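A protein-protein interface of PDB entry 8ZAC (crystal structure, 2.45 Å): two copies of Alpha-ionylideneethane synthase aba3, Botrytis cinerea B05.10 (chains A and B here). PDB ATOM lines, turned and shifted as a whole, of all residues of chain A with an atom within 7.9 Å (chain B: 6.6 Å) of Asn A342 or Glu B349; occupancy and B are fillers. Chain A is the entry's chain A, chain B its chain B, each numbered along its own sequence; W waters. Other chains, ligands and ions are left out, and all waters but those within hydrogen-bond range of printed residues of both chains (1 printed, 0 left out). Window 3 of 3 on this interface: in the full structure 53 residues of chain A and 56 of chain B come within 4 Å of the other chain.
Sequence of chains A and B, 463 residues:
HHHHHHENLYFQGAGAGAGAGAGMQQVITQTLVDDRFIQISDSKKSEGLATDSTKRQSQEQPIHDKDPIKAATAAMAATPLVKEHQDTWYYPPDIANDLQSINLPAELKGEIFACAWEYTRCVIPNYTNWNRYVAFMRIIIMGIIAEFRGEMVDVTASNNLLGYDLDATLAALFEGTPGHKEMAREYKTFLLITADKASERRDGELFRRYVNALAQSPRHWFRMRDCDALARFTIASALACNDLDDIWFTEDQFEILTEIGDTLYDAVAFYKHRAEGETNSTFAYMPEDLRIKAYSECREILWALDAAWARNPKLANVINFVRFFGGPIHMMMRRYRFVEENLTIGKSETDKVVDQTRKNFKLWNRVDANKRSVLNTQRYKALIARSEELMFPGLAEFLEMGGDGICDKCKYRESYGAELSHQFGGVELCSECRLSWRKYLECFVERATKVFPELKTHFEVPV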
ATOM      1  N   ARG A 337       4.092   6.490 -13.448  1.00  0.00           N
ATOM      2  CA  ARG A 337       4.512   6.806 -12.066  1.00  0.00           C
ATOM      3  C   ARG A 337       3.891   8.141 -11.601  1.00  0.00           C
ATOM      4  O   ARG A 337       4.504   8.848 -10.744  1.00  0.00           O
ATOM      5  CB  ARG A 337       6.044   6.753 -12.041  1.00  0.00           C
ATOM      6  CG  ARG A 337       6.583   5.327 -12.045  1.00  0.00           C
ATOM      7  CD  ARG A 337       8.085   5.228 -11.803  1.00  0.00           C
ATOM      8  NE  ARG A 337       8.464   5.294 -10.387  1.00  0.00           N
ATOM      9  CZ  ARG A 337       9.052   6.330  -9.778  1.00  0.00           C
ATOM     10  NH1 ARG A 337       9.340   7.441 -10.440  1.00  0.00           N
ATOM     11  NH2 ARG A 337       9.341   6.259  -8.488  1.00  0.00           N
ATOM     12  N   PHE A 338       2.698   8.490 -12.096  1.00  0.00           N
ATOM     13  CA  PHE A 338       2.033   9.767 -11.723  1.00  0.00           C
ATOM     14  C   PHE A 338       1.796   9.781 -10.197  1.00  0.00           C
ATOM     15  O   PHE A 338       2.095  10.794  -9.533  1.00  0.00           O
ATOM     16  CB  PHE A 338       0.747   9.932 -12.544  1.00  0.00           C
ATOM     17  CG  PHE A 338       0.101  11.282 -12.437  1.00  0.00           C
ATOM     18  CD1 PHE A 338       0.794  12.418 -12.799  1.00  0.00           C
ATOM     19  CD2 PHE A 338      -1.179  11.422 -11.949  1.00  0.00           C
ATOM     20  CE1 PHE A 338       0.207  13.666 -12.714  1.00  0.00           C
ATOM     21  CE2 PHE A 338      -1.758  12.674 -11.844  1.00  0.00           C
ATOM     22  CZ  PHE A 338      -1.064  13.794 -12.212  1.00  0.00           C
ATOM     23  N   VAL A 339       1.263   8.685  -9.652  1.00  0.00           N
ATOM     24  CA  VAL A 339       0.943   8.535  -8.204  1.00  0.00           C
ATOM     25  C   VAL A 339       2.250   8.529  -7.386  1.00  0.00           C
ATOM     26  O   VAL A 339       2.334   9.280  -6.429  1.00  0.00           O
ATOM     27  CB  VAL A 339       0.087   7.275  -7.990  1.00  0.00           C
ATOM     28  CG1 VAL A 339       0.149   6.800  -6.567  1.00  0.00           C
ATOM     29  CG2 VAL A 339      -1.375   7.482  -8.418  1.00  0.00           C
ATOM     30  N   GLU A 340       3.266   7.766  -7.793  1.00  0.00           N
ATOM     31  CA  GLU A 340       4.560   7.652  -7.073  1.00  0.00           C
ATOM     32  C   GLU A 340       5.266   9.005  -7.074  1.00  0.00           C
ATOM     33  O   GLU A 340       5.983   9.266  -6.116  1.00  0.00           O
ATOM     34  CB  GLU A 340       5.475   6.612  -7.719  1.00  0.00           C
ATOM     35  CG  GLU A 340       4.991   5.165  -7.568  1.00  0.00           C
ATOM     36  CD  GLU A 340       3.861   4.740  -8.494  1.00  0.00           C
ATOM     37  OE1 GLU A 340       3.407   5.574  -9.296  1.00  0.00           O
ATOM     38  OE2 GLU A 340       3.404   3.588  -8.379  1.00  0.00           O
ATOM     39  N   GLU A 341       5.048   9.850  -8.086  1.00  0.00           N
ATOM     40  CA  GLU A 341       5.714  11.173  -8.191  1.00  0.00           C
ATOM     41  C   GLU A 341       4.780  12.270  -7.668  1.00  0.00           C
ATOM     42  O   GLU A 341       4.980  13.445  -8.061  1.00  0.00           O
ATOM     43  CB  GLU A 341       6.192  11.427  -9.624  1.00  0.00           C
ATOM     44  CG  GLU A 341       7.236  10.421 -10.104  1.00  0.00           C
ATOM     45  CD  GLU A 341       7.640  10.479 -11.577  1.00  0.00           C
ATOM     46  OE1 GLU A 341       6.896  11.064 -12.402  1.00  0.00           O
ATOM     47  OE2 GLU A 341       8.708   9.922 -11.914  1.00  0.00           O
ATOM     48  N   ASN A 342       3.811  11.901  -6.811  1.00  0.00           N
ATOM     49  CA  ASN A 342       2.869  12.804  -6.068  1.00  0.00           C
ATOM     50  C   ASN A 342       2.030  13.671  -7.031  1.00  0.00           C
ATOM     51  O   ASN A 342       1.941  14.878  -6.802  1.00  0.00           O
ATOM     52  CB  ASN A 342       3.599  13.612  -4.986  1.00  0.00           C
ATOM     53  CG  ASN A 342       4.430  12.727  -4.065  1.00  0.00           C
ATOM     54  OD1 ASN A 342       3.914  11.801  -3.419  1.00  0.00           O
ATOM     55  ND2 ASN A 342       5.736  12.978  -4.018  1.00  0.00           N
ATOM     56  N   LEU A 343       1.410  13.039  -8.041  1.00  0.00           N
ATOM     57  CA  LEU A 343       0.505  13.640  -9.066  1.00  0.00           C
ATOM     58  C   LEU A 343       1.199  14.819  -9.735  1.00  0.00           C
ATOM     59  O   LEU A 343       0.557  15.868  -9.927  1.00  0.00           O
ATOM     60  CB  LEU A 343      -0.805  14.081  -8.408  1.00  0.00           C
ATOM     61  CG  LEU A 343      -1.486  13.061  -7.501  1.00  0.00           C
ATOM     62  CD1 LEU A 343      -2.838  13.575  -7.099  1.00  0.00           C
ATOM     63  CD2 LEU A 343      -1.629  11.715  -8.178  1.00  0.00           C
ATOM     64  N   THR A 344       2.467  14.636 -10.086  1.00  0.00           N
ATOM     65  CA  THR A 344       3.255  15.573 -10.913  1.00  0.00           C
ATOM     66  C   THR A 344       3.591  14.881 -12.233  1.00  0.00           C
ATOM     67  O   THR A 344       3.670  13.637 -12.276  1.00  0.00           O
ATOM     68  CB  THR A 344       4.518  16.061 -10.180  1.00  0.00           C
ATOM     69  OG1 THR A 344       5.394  14.954  -9.952  1.00  0.00           O
ATOM     70  CG2 THR A 344       4.217  16.758  -8.867  1.00  0.00           C
ATOM     71  N   ILE A 345       3.826  15.688 -13.259  1.00  0.00           N
ATOM     72  CA  ILE A 345       4.466  15.269 -14.538  1.00  0.00           C
ATOM     73  C   ILE A 345       5.678  16.169 -14.793  1.00  0.00           C
ATOM     74  O   ILE A 345       5.533  17.410 -14.636  1.00  0.00           O
ATOM     75  CB  ILE A 345       3.439  15.330 -15.679  1.00  0.00           C
ATOM     76  CG1 ILE A 345       2.550  14.084 -15.628  1.00  0.00           C
ATOM     77  CG2 ILE A 345       4.129  15.522 -17.025  1.00  0.00           C
ATOM     78  CD1 ILE A 345       1.426  14.104 -16.616  1.00  0.00           C
ATOM     79  N   LYS A 347       8.745  16.375 -13.294  1.00  0.00           N
ATOM     80  CA  LYS A 347       9.229  17.053 -12.051  1.00  0.00           C
ATOM     81  C   LYS A 347       9.949  16.058 -11.124  1.00  0.00           C
ATOM     82  O   LYS A 347       9.877  16.264  -9.886  1.00  0.00           O
ATOM     83  CB  LYS A 347       8.060  17.715 -11.305  1.00  0.00           C
ATOM     84  CG  LYS A 347       7.527  18.998 -11.930  1.00  0.00           C
ATOM     85  CD  LYS A 347       7.119  20.054 -10.914  1.00  0.00           C
ATOM     86  CE  LYS A 347       6.955  21.425 -11.527  1.00  0.00           C
ATOM     87  NZ  LYS A 347       6.514  22.430 -10.532  1.00  0.00           N
ATOM     88  N   ALA B 267      -7.616  16.575  -6.783  1.00  0.00           N
ATOM     89  CA  ALA B 267      -6.291  15.996  -6.484  1.00  0.00           C
ATOM     90  C   ALA B 267      -5.251  16.555  -7.474  1.00  0.00           C
ATOM     91  O   ALA B 267      -4.162  16.978  -7.032  1.00  0.00           O
ATOM     92  CB  ALA B 267      -6.365  14.489  -6.519  1.00  0.00           C
ATOM     93  N   TYR B 271      -2.601  22.383  -6.234  1.00  0.00           N
ATOM     94  CA  TYR B 271      -1.617  23.495  -6.144  1.00  0.00           C
ATOM     95  C   TYR B 271      -2.093  24.699  -6.983  1.00  0.00           C
ATOM     96  O   TYR B 271      -1.707  25.845  -6.655  1.00  0.00           O
ATOM     97  CB  TYR B 271      -0.201  23.030  -6.518  1.00  0.00           C
ATOM     98  CG  TYR B 271       0.426  22.087  -5.518  1.00  0.00           C
ATOM     99  CD1 TYR B 271       0.592  22.463  -4.188  1.00  0.00           C
ATOM    100  CD2 TYR B 271       0.853  20.815  -5.887  1.00  0.00           C
ATOM    101  CE1 TYR B 271       1.153  21.609  -3.249  1.00  0.00           C
ATOM    102  CE2 TYR B 271       1.413  19.951  -4.959  1.00  0.00           C
ATOM    103  CZ  TYR B 271       1.558  20.341  -3.634  1.00  0.00           C
ATOM    104  OH  TYR B 271       2.082  19.487  -2.693  1.00  0.00           O
ATOM    105  N   ARG B 291      -4.593  13.213  -0.216  1.00  0.00           N
ATOM    106  CA  ARG B 291      -4.707  13.581  -1.669  1.00  0.00           C
ATOM    107  C   ARG B 291      -4.194  12.465  -2.591  1.00  0.00           C
ATOM    108  O   ARG B 291      -4.934  12.062  -3.521  1.00  0.00           O
ATOM    109  CB  ARG B 291      -3.907  14.847  -1.975  1.00  0.00           C
ATOM    110  CG  ARG B 291      -4.057  15.347  -3.398  1.00  0.00           C
ATOM    111  CD  ARG B 291      -3.620  16.771  -3.492  1.00  0.00           C
ATOM    112  NE  ARG B 291      -2.174  16.895  -3.379  1.00  0.00           N
ATOM    113  CZ  ARG B 291      -1.328  16.916  -4.414  1.00  0.00           C
ATOM    114  NH1 ARG B 291      -1.765  16.798  -5.662  1.00  0.00           N
ATOM    115  NH2 ARG B 291      -0.033  17.057  -4.199  1.00  0.00           N
ATOM    116  N   ILE B 292      -2.979  11.973  -2.347  1.00  0.00           N
ATOM    117  CA  ILE B 292      -2.320  10.941  -3.203  1.00  0.00           C
ATOM    118  C   ILE B 292      -3.094   9.618  -3.089  1.00  0.00           C
ATOM    119  O   ILE B 292      -3.318   8.986  -4.138  1.00  0.00           O
ATOM    120  CB  ILE B 292      -0.820  10.788  -2.855  1.00  0.00           C
ATOM    121  CG1 ILE B 292      -0.075  12.118  -2.959  1.00  0.00           C
ATOM    122  CG2 ILE B 292      -0.150   9.716  -3.707  1.00  0.00           C
ATOM    123  CD1 ILE B 292      -0.021  12.684  -4.322  1.00  0.00           C
ATOM    124  N   ILE B 345       2.958  19.141 -14.694  1.00  0.00           N
ATOM    125  CA  ILE B 345       1.766  19.266 -13.821  1.00  0.00           C
ATOM    126  C   ILE B 345       2.240  19.208 -12.360  1.00  0.00           C
ATOM    127  O   ILE B 345       3.094  18.378 -12.013  1.00  0.00           O
ATOM    128  CB  ILE B 345       0.713  18.203 -14.219  1.00  0.00           C
ATOM    129  CG1 ILE B 345      -0.175  18.713 -15.362  1.00  0.00           C
ATOM    130  CG2 ILE B 345      -0.147  17.771 -13.048  1.00  0.00           C
ATOM    131  CD1 ILE B 345      -0.302  17.744 -16.492  1.00  0.00           C
ATOM    132  N   GLY B 346       1.700  20.084 -11.524  1.00  0.00           N
ATOM    133  CA  GLY B 346       1.885  19.999 -10.069  1.00  0.00           C
ATOM    134  C   GLY B 346       3.227  20.519  -9.602  1.00  0.00           C
ATOM    135  O   GLY B 346       3.899  21.287 -10.324  1.00  0.00           O
ATOM    136  N   LYS B 347       3.581  20.124  -8.387  1.00  0.00           N
ATOM    137  CA  LYS B 347       4.718  20.663  -7.605  1.00  0.00           C
ATOM    138  C   LYS B 347       5.375  19.468  -6.932  1.00  0.00           C
ATOM    139  O   LYS B 347       4.645  18.711  -6.270  1.00  0.00           O
ATOM    140  CB  LYS B 347       4.221  21.678  -6.565  1.00  0.00           C
ATOM    141  CG  LYS B 347       3.651  22.979  -7.116  1.00  0.00           C
ATOM    142  CD  LYS B 347       4.733  23.986  -7.487  1.00  0.00           C
ATOM    143  CE  LYS B 347       4.226  25.177  -8.275  1.00  0.00           C
ATOM    144  NZ  LYS B 347       5.126  25.510  -9.409  1.00  0.00           N
ATOM    145  N   SER B 348       6.678  19.279  -7.125  1.00  0.00           N
ATOM    146  CA  SER B 348       7.466  18.219  -6.449  1.00  0.00           C
ATOM    147  C   SER B 348       7.563  18.565  -4.958  1.00  0.00           C
ATOM    148  O   SER B 348       7.197  19.703  -4.574  1.00  0.00           O
ATOM    149  CB  SER B 348       8.820  18.076  -7.073  1.00  0.00           C
ATOM    150  OG  SER B 348       9.507  19.318  -7.045  1.00  0.00           O
ATOM    151  N   GLU B 349       8.060  17.627  -4.151  1.00  0.00           N
ATOM    152  CA  GLU B 349       8.258  17.823  -2.690  1.00  0.00           C
ATOM    153  C   GLU B 349       9.332  18.889  -2.431  1.00  0.00           C
ATOM    154  O   GLU B 349       9.270  19.522  -1.355  1.00  0.00           O
ATOM    155  CB  GLU B 349       8.617  16.497  -2.021  1.00  0.00           C
ATOM    156  CG  GLU B 349       7.425  15.848  -1.341  1.00  0.00           C
ATOM    157  CD  GLU B 349       7.333  14.339  -1.489  1.00  0.00           C
ATOM    158  OE1 GLU B 349       8.046  13.772  -2.358  1.00  0.00           O
ATOM    159  OE2 GLU B 349       6.548  13.735  -0.726  1.00  0.00           O
ATOM    160  N   THR B 350      10.260  19.089  -3.376  1.00  0.00           N
ATOM    161  CA  THR B 350      11.439  19.988  -3.231  1.00  0.00           C
ATOM    162  C   THR B 350      11.248  21.254  -4.088  1.00  0.00           C
ATOM    163  O   THR B 350      12.277  21.849  -4.480  1.00  0.00           O
ATOM    164  CB  THR B 350      12.738  19.214  -3.521  1.00  0.00           C
ATOM    165  OG1 THR B 350      12.638  18.609  -4.812  1.00  0.00           O
ATOM    166  CG2 THR B 350      13.029  18.128  -2.503  1.00  0.00           C
ATOM    167  N   ASP B 351       9.997  21.683  -4.330  1.00  0.00           N
ATOM    168  CA  ASP B 351       9.657  22.878  -5.156  1.00  0.00           C
ATOM    169  C   ASP B 351       9.154  24.010  -4.261  1.00  0.00           C
ATOM    170  O   ASP B 351       8.567  23.716  -3.210  1.00  0.00           O
ATOM    171  CB  ASP B 351       8.581  22.589  -6.209  1.00  0.00           C
ATOM    172  CG  ASP B 351       9.065  22.499  -7.649  1.00  0.00           C
ATOM    173  OD1 ASP B 351      10.169  23.023  -7.959  1.00  0.00           O
ATOM    174  OD2 ASP B 351       8.319  21.908  -8.459  1.00  0.00           O
HETATM  175  O   HOH W   1      -0.110  17.730  -7.822  1.00  0.00           O
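Of the 10 printed residues of chain A, 6 touch a printed residue of chain B. Among the printed residues, Asp or Glu carboxylates within 4 Å of a Lys or Arg side-chain nitrogen of the other chain: Lys A347 with Asp B351 (2.8 Å).
Among the printed residues, merely in contact across the chains: Val A339 with Ile B292 (3.7 Å), Asn A342 with Arg B291 (3.9 Å), Asn A342 with Ile B292 (3.4 Å), Leu A343 with Ala B267 (3.7 Å), Leu A343 with Arg B291 (3.7 Å), Leu A343 with Ile B292 (3.5 Å), Leu A343 with Ile B345 (3.7 Å), Thr A344 with Ile B345 (3.0 Å), Thr A344 with Gly B346 (3.96 Å), Thr A344 with Lys B347 (3.3 Å), Thr A344 with Ser B348 (3.9 Å), Lys A347 with Lys B347 (3.6 Å) and Lys A347 with Ser B348 (3.5 Å).
The side-chain carboxylate (OD2) of Asp B351 sits at hydrogen-bond distance from the side-chain hydroxyl (OG) of Ser B348 (3.2 Å). O of Ala B267 sits at hydrogen-bond distance from NH1 of Arg B291, 2.8 Å away. The backbone carbonyl oxygen of Phe A338 lies within hydrogen-bond range of the backbone NH of Leu A343, at 2.8 Å. O of Glu A341 sits at hydrogen-bond distance from OG1 of Thr A344, 2.5 Å away.
O of Gly B346 sits at hydrogen-bond distance from NZ of Lys A347, at 2.9 Å. The backbone NH (N) of Ile A345 sits at hydrogen-bond distance from the backbone carbonyl oxygen (O) of Ile B345 (3.1 Å). OE1 of Glu B349 is in hydrogen-bond range of ND2 of Asn A342, at 3.0 Å. The side-chain carboxylate (OD2) of Asp B351 lies within salt-bridge range of the side-chain amino group (NZ) of Lys A347 (2.8 Å).
Ile A345 touches its own counterpart, Ile B345. Lys A347 touches its own counterpart, Lys B347. 2 positions are printed for both chains.
Of the printed residues of chain B, Val A339 touches Ile B292 (3.7 Å). Of chain B, only Arg B291, Ile B292 and Glu B349 come within 4 Å of Asn A342. Of the printed residues of chain B, Lys A347 touches Gly B346, Lys B347, Ser B348 and Asp B351. Printed residues of chain A within 4 Å of Ala B267: Leu A343 (3.7 Å). Of the printed residues of chain A, Gly B346 touches Thr A344 and Lys A347. Of the printed residues of chain A, Lys B347 touches Thr A344 (3.3 Å) and Lys A347 (3.6 Å). Of chain A, only Thr A344 (3.9 Å) and Lys A347 (3.5 Å) come within 4 Å of Ser B348. The nearest residue of chain B that does not touch Asn A342 is Lys B347 (4.7 Å). The nearest printed residue of chain B that does not touch Lys A347 is Ile B345 (4.5 Å).
Water W1 bridges NH1 of Arg B291 and O of Leu A343.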
